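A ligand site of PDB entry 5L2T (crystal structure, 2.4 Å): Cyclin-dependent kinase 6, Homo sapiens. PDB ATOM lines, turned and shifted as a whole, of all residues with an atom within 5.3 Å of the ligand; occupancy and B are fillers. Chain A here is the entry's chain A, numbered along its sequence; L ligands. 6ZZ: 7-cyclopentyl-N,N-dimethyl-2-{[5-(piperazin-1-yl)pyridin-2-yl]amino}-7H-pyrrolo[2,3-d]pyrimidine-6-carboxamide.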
ATOM      1  N   ILE A  19     -18.822 -23.765 -25.885  1.00  0.00           N
ATOM      2  CA  ILE A  19     -18.508 -22.745 -24.870  1.00  0.00           C
ATOM      3  C   ILE A  19     -17.483 -21.753 -25.441  1.00  0.00           C
ATOM      4  O   ILE A  19     -17.836 -20.594 -25.707  1.00  0.00           O
ATOM      5  CB  ILE A  19     -18.143 -23.332 -23.472  1.00  0.00           C
ATOM      6  CG1 ILE A  19     -19.326 -24.172 -22.879  1.00  0.00           C
ATOM      7  CG2 ILE A  19     -17.691 -22.248 -22.509  1.00  0.00           C
ATOM      8  CD1 ILE A  19     -20.564 -23.409 -22.299  1.00  0.00           C
ATOM      9  N   GLY A  20     -16.269 -22.221 -25.678  1.00  0.00           N
ATOM     10  CA  GLY A  20     -15.216 -21.436 -26.322  1.00  0.00           C
ATOM     11  C   GLY A  20     -14.595 -22.295 -27.402  1.00  0.00           C
ATOM     12  O   GLY A  20     -15.306 -22.995 -28.138  1.00  0.00           O
ATOM     13  N   VAL A  27     -15.821 -28.097 -25.637  1.00  0.00           N
ATOM     14  CA  VAL A  27     -16.700 -27.942 -24.474  1.00  0.00           C
ATOM     15  C   VAL A  27     -18.049 -27.453 -24.971  1.00  0.00           C
ATOM     16  O   VAL A  27     -18.130 -26.451 -25.696  1.00  0.00           O
ATOM     17  CB  VAL A  27     -16.126 -27.015 -23.343  1.00  0.00           C
ATOM     18  CG1 VAL A  27     -17.013 -27.032 -22.098  1.00  0.00           C
ATOM     19  CG2 VAL A  27     -14.708 -27.398 -22.977  1.00  0.00           C
ATOM     20  N   ALA A  41     -22.147 -28.047 -18.591  1.00  0.00           N
ATOM     21  CA  ALA A  41     -20.962 -27.907 -19.415  1.00  0.00           C
ATOM     22  C   ALA A  41     -20.426 -29.313 -19.600  1.00  0.00           C
ATOM     23  O   ALA A  41     -20.146 -30.010 -18.637  1.00  0.00           O
ATOM     24  CB  ALA A  41     -19.931 -27.026 -18.740  1.00  0.00           C
ATOM     25  N   LYS A  43     -17.675 -31.886 -21.523  1.00  0.00           N
ATOM     26  CA  LYS A  43     -16.333 -31.945 -22.113  1.00  0.00           C
ATOM     27  C   LYS A  43     -15.958 -33.403 -22.328  1.00  0.00           C
ATOM     28  O   LYS A  43     -16.122 -34.221 -21.434  1.00  0.00           O
ATOM     29  CB  LYS A  43     -15.290 -31.231 -21.233  1.00  0.00           C
ATOM     30  CG  LYS A  43     -14.013 -30.892 -22.017  1.00  0.00           C
ATOM     31  CD  LYS A  43     -12.763 -30.772 -21.157  1.00  0.00           C
ATOM     32  CE  LYS A  43     -11.571 -30.376 -21.984  1.00  0.00           C
ATOM     33  NZ  LYS A  43     -11.611 -28.947 -22.403  1.00  0.00           N
ATOM     34  N   VAL A  77     -15.887 -24.904  -9.561  1.00  0.00           N
ATOM     35  CA  VAL A  77     -16.984 -25.377 -10.410  1.00  0.00           C
ATOM     36  C   VAL A  77     -17.412 -26.820 -10.042  1.00  0.00           C
ATOM     37  O   VAL A  77     -16.566 -27.703  -9.934  1.00  0.00           O
ATOM     38  CB  VAL A  77     -16.637 -25.206 -11.921  1.00  0.00           C
ATOM     39  CG1 VAL A  77     -15.516 -26.164 -12.371  1.00  0.00           C
ATOM     40  CG2 VAL A  77     -17.877 -25.377 -12.796  1.00  0.00           C
ATOM     41  N   LEU A  96     -17.191 -35.576 -19.290  1.00  0.00           N
ATOM     42  CA  LEU A  96     -17.244 -34.791 -18.045  1.00  0.00           C
ATOM     43  C   LEU A  96     -18.405 -33.808 -18.013  1.00  0.00           C
ATOM     44  O   LEU A  96     -18.482 -32.913 -18.835  1.00  0.00           O
ATOM     45  CB  LEU A  96     -15.920 -34.018 -17.867  1.00  0.00           C
ATOM     46  CG  LEU A  96     -14.891 -34.541 -16.852  1.00  0.00           C
ATOM     47  CD1 LEU A  96     -14.469 -35.969 -17.139  1.00  0.00           C
ATOM     48  CD2 LEU A  96     -13.649 -33.697 -16.897  1.00  0.00           C
ATOM     49  N   PHE A  98     -20.266 -30.893 -15.916  1.00  0.00           N
ATOM     50  CA  PHE A  98     -20.115 -29.887 -14.859  1.00  0.00           C
ATOM     51  C   PHE A  98     -21.378 -29.055 -14.820  1.00  0.00           C
ATOM     52  O   PHE A  98     -22.128 -29.037 -15.794  1.00  0.00           O
ATOM     53  CB  PHE A  98     -18.945 -28.948 -15.177  1.00  0.00           C
ATOM     54  CG  PHE A  98     -17.568 -29.567 -15.212  1.00  0.00           C
ATOM     55  CD1 PHE A  98     -16.749 -29.566 -14.089  1.00  0.00           C
ATOM     56  CD2 PHE A  98     -17.051 -30.076 -16.401  1.00  0.00           C
ATOM     57  CE1 PHE A  98     -15.458 -30.095 -14.137  1.00  0.00           C
ATOM     58  CE2 PHE A  98     -15.774 -30.635 -16.432  1.00  0.00           C
ATOM     59  CZ  PHE A  98     -14.987 -30.625 -15.309  1.00  0.00           C
ATOM     60  N   GLU A  99     -21.570 -28.268 -13.739  1.00  0.00           N
ATOM     61  CA  GLU A  99     -22.653 -27.298 -13.701  1.00  0.00           C
ATOM     62  C   GLU A  99     -22.354 -26.257 -14.828  1.00  0.00           C
ATOM     63  O   GLU A  99     -21.252 -26.249 -15.364  1.00  0.00           O
ATOM     64  CB  GLU A  99     -22.696 -26.596 -12.331  1.00  0.00           C
ATOM     65  CG  GLU A  99     -21.458 -25.761 -12.049  1.00  0.00           C
ATOM     66  CD  GLU A  99     -21.510 -24.918 -10.807  1.00  0.00           C
ATOM     67  OE1 GLU A  99     -20.526 -24.929 -10.040  1.00  0.00           O
ATOM     68  OE2 GLU A  99     -22.539 -24.228 -10.606  1.00  0.00           O
ATOM     69  N   HIS A 100     -23.328 -25.445 -15.218  1.00  0.00           N
ATOM     70  CA  HIS A 100     -23.070 -24.419 -16.231  1.00  0.00           C
ATOM     71  C   HIS A 100     -23.181 -23.054 -15.582  1.00  0.00           C
ATOM     72  O   HIS A 100     -24.047 -22.863 -14.723  1.00  0.00           O
ATOM     73  CB  HIS A 100     -24.048 -24.540 -17.411  1.00  0.00           C
ATOM     74  CG  HIS A 100     -23.860 -23.458 -18.441  1.00  0.00           C
ATOM     75  ND1 HIS A 100     -24.675 -22.324 -18.459  1.00  0.00           N
ATOM     76  CD2 HIS A 100     -22.920 -23.336 -19.410  1.00  0.00           C
ATOM     77  CE1 HIS A 100     -24.218 -21.576 -19.451  1.00  0.00           C
ATOM     78  NE2 HIS A 100     -23.162 -22.144 -20.042  1.00  0.00           N
ATOM     79  N   VAL A 101     -22.286 -22.123 -15.918  1.00  0.00           N
ATOM     80  CA  VAL A 101     -22.420 -20.755 -15.435  1.00  0.00           C
ATOM     81  C   VAL A 101     -22.295 -19.852 -16.676  1.00  0.00           C
ATOM     82  O   VAL A 101     -21.536 -20.133 -17.607  1.00  0.00           O
ATOM     83  CB  VAL A 101     -21.646 -20.326 -14.143  1.00  0.00           C
ATOM     84  CG1 VAL A 101     -20.811 -21.429 -13.527  1.00  0.00           C
ATOM     85  CG2 VAL A 101     -20.889 -19.011 -14.275  1.00  0.00           C
ATOM     86  N   ASP A 102     -23.230 -18.896 -16.756  1.00  0.00           N
ATOM     87  CA  ASP A 102     -23.456 -17.984 -17.883  1.00  0.00           C
ATOM     88  C   ASP A 102     -22.291 -17.119 -18.251  1.00  0.00           C
ATOM     89  O   ASP A 102     -22.058 -16.936 -19.442  1.00  0.00           O
ATOM     90  CB  ASP A 102     -24.697 -17.104 -17.618  1.00  0.00           C
ATOM     91  CG  ASP A 102     -26.030 -17.794 -17.762  1.00  0.00           C
ATOM     92  OD1 ASP A 102     -26.361 -18.221 -18.894  1.00  0.00           O
ATOM     93  OD2 ASP A 102     -26.778 -17.851 -16.753  1.00  0.00           O
ATOM     94  N   GLN A 103     -21.613 -16.517 -17.266  1.00  0.00           N
ATOM     95  CA  GLN A 103     -20.510 -15.639 -17.614  1.00  0.00           C
ATOM     96  C   GLN A 103     -19.191 -16.040 -16.952  1.00  0.00           C
ATOM     97  O   GLN A 103     -19.172 -16.749 -15.950  1.00  0.00           O
ATOM     98  CB  GLN A 103     -20.893 -14.144 -17.381  1.00  0.00           C
ATOM     99  CG  GLN A 103     -20.799 -13.639 -15.953  1.00  0.00           C
ATOM    100  CD  GLN A 103     -21.596 -12.379 -15.699  1.00  0.00           C
ATOM    101  OE1 GLN A 103     -21.316 -11.303 -16.252  1.00  0.00           O
ATOM    102  NE2 GLN A 103     -22.564 -12.473 -14.804  1.00  0.00           N
ATOM    103  N   ASP A 104     -18.098 -15.610 -17.592  1.00  0.00           N
ATOM    104  CA  ASP A 104     -16.721 -15.735 -17.129  1.00  0.00           C
ATOM    105  C   ASP A 104     -16.392 -14.317 -16.651  1.00  0.00           C
ATOM    106  O   ASP A 104     -17.202 -13.414 -16.886  1.00  0.00           O
ATOM    107  CB  ASP A 104     -15.800 -16.213 -18.268  1.00  0.00           C
ATOM    108  CG  ASP A 104     -15.687 -15.294 -19.482  1.00  0.00           C
ATOM    109  OD1 ASP A 104     -16.544 -14.398 -19.637  1.00  0.00           O
ATOM    110  OD2 ASP A 104     -14.749 -15.478 -20.285  1.00  0.00           O
ATOM    111  N   THR A 107     -16.420 -11.414 -19.601  1.00  0.00           N
ATOM    112  CA  THR A 107     -17.707 -10.825 -19.989  1.00  0.00           C
ATOM    113  C   THR A 107     -18.307 -10.011 -18.847  1.00  0.00           C
ATOM    114  O   THR A 107     -19.031  -9.051 -19.109  1.00  0.00           O
ATOM    115  CB  THR A 107     -18.638 -11.849 -20.579  1.00  0.00           C
ATOM    116  OG1 THR A 107     -18.812 -12.880 -19.632  1.00  0.00           O
ATOM    117  CG2 THR A 107     -18.090 -12.458 -21.857  1.00  0.00           C
ATOM    118  N   GLN A 149     -10.990 -15.837 -18.324  1.00  0.00           N
ATOM    119  CA  GLN A 149     -11.745 -16.672 -19.246  1.00  0.00           C
ATOM    120  C   GLN A 149     -12.177 -17.969 -18.646  1.00  0.00           C
ATOM    121  O   GLN A 149     -13.103 -18.582 -19.164  1.00  0.00           O
ATOM    122  CB  GLN A 149     -10.938 -16.931 -20.533  1.00  0.00           C
ATOM    123  CG  GLN A 149     -10.883 -15.730 -21.499  1.00  0.00           C
ATOM    124  CD  GLN A 149      -9.846 -14.678 -21.139  1.00  0.00           C
ATOM    125  OE1 GLN A 149      -9.863 -13.556 -21.658  1.00  0.00           O
ATOM    126  NE2 GLN A 149      -8.905 -15.001 -20.240  1.00  0.00           N
ATOM    127  N   ASN A 150     -11.480 -18.438 -17.588  1.00  0.00           N
ATOM    128  CA  ASN A 150     -11.886 -19.668 -16.908  1.00  0.00           C
ATOM    129  C   ASN A 150     -12.357 -19.427 -15.443  1.00  0.00           C
ATOM    130  O   ASN A 150     -12.630 -20.377 -14.726  1.00  0.00           O
ATOM    131  CB  ASN A 150     -10.842 -20.793 -17.013  1.00  0.00           C
ATOM    132  CG  ASN A 150      -9.438 -20.437 -16.645  1.00  0.00           C
ATOM    133  OD1 ASN A 150      -9.150 -19.740 -15.660  1.00  0.00           O
ATOM    134  ND2 ASN A 150      -8.545 -20.958 -17.453  1.00  0.00           N
ATOM    135  N   LEU A 152     -15.416 -18.338 -13.374  1.00  0.00           N
ATOM    136  CA  LEU A 152     -16.849 -18.201 -13.603  1.00  0.00           C
ATOM    137  C   LEU A 152     -17.502 -17.264 -12.602  1.00  0.00           C
ATOM    138  O   LEU A 152     -17.191 -17.293 -11.417  1.00  0.00           O
ATOM    139  CB  LEU A 152     -17.515 -19.566 -13.595  1.00  0.00           C
ATOM    140  CG  LEU A 152     -16.783 -20.683 -14.325  1.00  0.00           C
ATOM    141  CD1 LEU A 152     -17.377 -22.011 -13.978  1.00  0.00           C
ATOM    142  CD2 LEU A 152     -16.732 -20.454 -15.813  1.00  0.00           C
ATOM    143  N   ALA A 162     -12.496 -22.859 -12.612  1.00  0.00           N
ATOM    144  CA  ALA A 162     -12.793 -23.893 -13.600  1.00  0.00           C
ATOM    145  C   ALA A 162     -11.574 -24.186 -14.502  1.00  0.00           C
ATOM    146  O   ALA A 162     -10.608 -23.419 -14.486  1.00  0.00           O
ATOM    147  CB  ALA A 162     -13.982 -23.462 -14.452  1.00  0.00           C
ATOM    148  N   ASP A 163     -11.639 -25.287 -15.259  1.00  0.00           N
ATOM    149  CA  ASP A 163     -10.666 -25.696 -16.279  1.00  0.00           C
ATOM    150  C   ASP A 163      -9.224 -25.903 -15.767  1.00  0.00           C
ATOM    151  O   ASP A 163      -8.273 -25.320 -16.296  1.00  0.00           O
ATOM    152  CB  ASP A 163     -10.716 -24.674 -17.448  1.00  0.00           C
ATOM    153  CG  ASP A 163     -10.473 -25.235 -18.833  1.00  0.00           C
ATOM    154  OD1 ASP A 163     -10.557 -26.481 -18.995  1.00  0.00           O
ATOM    155  OD2 ASP A 163     -10.219 -24.445 -19.748  1.00  0.00           O
ATOM    156  N   PHE A 164      -9.079 -26.709 -14.705  1.00  0.00           N
ATOM    157  CA  PHE A 164      -7.814 -27.067 -14.023  1.00  0.00           C
ATOM    158  C   PHE A 164      -7.773 -28.586 -13.798  1.00  0.00           C
ATOM    159  O   PHE A 164      -8.806 -29.253 -13.894  1.00  0.00           O
ATOM    160  CB  PHE A 164      -7.723 -26.339 -12.662  1.00  0.00           C
ATOM    161  CG  PHE A 164      -8.848 -26.699 -11.720  1.00  0.00           C
ATOM    162  CD1 PHE A 164      -8.733 -27.777 -10.852  1.00  0.00           C
ATOM    163  CD2 PHE A 164     -10.032 -25.980 -11.721  1.00  0.00           C
ATOM    164  CE1 PHE A 164      -9.808 -28.150 -10.030  1.00  0.00           C
ATOM    165  CE2 PHE A 164     -11.094 -26.327 -10.885  1.00  0.00           C
ATOM    166  CZ  PHE A 164     -10.977 -27.424 -10.058  1.00  0.00           C
HETATM  167  C2  6ZZ L   1     -18.613 -22.508 -18.183  1.00  0.00           C
HETATM  168  C4  6ZZ L   1     -19.016 -24.134 -16.643  1.00  0.00           C
HETATM  169  C5  6ZZ L   1     -17.777 -24.739 -16.852  1.00  0.00           C
HETATM  170  C6  6ZZ L   1     -17.034 -24.079 -17.858  1.00  0.00           C
HETATM  171  C20 6ZZ L   1     -18.622 -19.019 -21.354  1.00  0.00           C
HETATM  172  N   6ZZ L   1     -19.204 -19.843 -20.463  1.00  0.00           N
HETATM  173  C9  6ZZ L   1     -16.992 -25.813 -16.382  1.00  0.00           C
HETATM  174  C18 6ZZ L   1     -16.477 -19.274 -20.359  1.00  0.00           C
HETATM  175  C19 6ZZ L   1     -17.257 -18.705 -21.356  1.00  0.00           C
HETATM  176  C8  6ZZ L   1     -15.809 -25.807 -17.071  1.00  0.00           C
HETATM  177  C16 6ZZ L   1     -18.416 -20.396 -19.528  1.00  0.00           C
HETATM  178  C10 6ZZ L   1     -14.650 -26.735 -16.907  1.00  0.00           C
HETATM  179  C24 6ZZ L   1     -13.492 -22.336 -19.612  1.00  0.00           C
HETATM  180  C25 6ZZ L   1     -14.325 -22.836 -20.741  1.00  0.00           C
HETATM  181  C23 6ZZ L   1     -14.121 -22.876 -18.364  1.00  0.00           C
HETATM  182  C26 6ZZ L   1     -14.900 -24.189 -20.291  1.00  0.00           C
HETATM  183  C28 6ZZ L   1     -15.657 -18.410 -23.201  1.00  0.00           C
HETATM  184  C32 6ZZ L   1     -17.442 -16.756 -22.904  1.00  0.00           C
HETATM  185  C29 6ZZ L   1     -14.702 -17.316 -23.612  1.00  0.00           C
HETATM  186  C31 6ZZ L   1     -16.508 -15.647 -23.334  1.00  0.00           C
HETATM  187  C22 6ZZ L   1     -14.646 -24.253 -18.784  1.00  0.00           C
HETATM  188  C13 6ZZ L   1     -13.301 -28.597 -17.773  1.00  0.00           C
HETATM  189  C14 6ZZ L   1     -15.225 -27.775 -19.057  1.00  0.00           C
HETATM  190  C   6ZZ L   1     -17.050 -20.120 -19.431  1.00  0.00           C
HETATM  191  N1  6ZZ L   1     -19.461 -23.052 -17.294  1.00  0.00           N
HETATM  192  N3  6ZZ L   1     -17.403 -22.992 -18.537  1.00  0.00           N
HETATM  193  N7  6ZZ L   1     -15.814 -24.729 -17.997  1.00  0.00           N
HETATM  194  N27 6ZZ L   1     -16.688 -17.863 -22.315  1.00  0.00           N
HETATM  195  N15 6ZZ L   1     -19.014 -21.291 -18.649  1.00  0.00           N
HETATM  196  N11 6ZZ L   1     -14.409 -27.641 -17.858  1.00  0.00           N
HETATM  197  N30 6ZZ L   1     -15.449 -16.183 -24.242  1.00  0.00           N
HETATM  198  O12 6ZZ L   1     -14.009 -26.686 -15.857  1.00  0.00           O
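N of Asp 163 is in hydrogen-bond range of O12 of the ligand, at 2.8 Å. A nitrogen (N1) of the ligand is in hydrogen-bond range of the backbone NH (N) of Val 101 (3.3 Å). O of Val 101 lies close to N15 of the ligand (3.0 Å).
The backbone carbonyl oxygen (O) of Ala 41 is in hydrogen-bond range of the backbone NH (N) of Phe 98 (2.9 Å). O of Val 27 is in hydrogen-bond range of N of Ile 19, 2.8 Å away. The backbone NH (N) of Ala 162 lies within hydrogen-bond range of the backbone carbonyl oxygen (O) of Asn 150, at 3.3 Å. The side-chain hydroxyl (OG1) of Thr 107 lies within hydrogen-bond range of the side-chain carboxylate (OD1) of Asp 104.
Merely in contact with the ligand: Glu 99 (3.3 Å), Phe 98 (3.5 Å), Ile 19 (3.5 Å), Ala 162 (3.5 Å), Asp 104 (3.5 Å), Val 27 (3.6 Å), Gln 149 (3.6 Å), Leu 152 (3.6 Å), Ala 41 (3.7 Å), Val 77 (3.7 Å) and Thr 107 (3.9 Å). Of the 21 residues printed, 13 come within 4 Å of the ligand.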
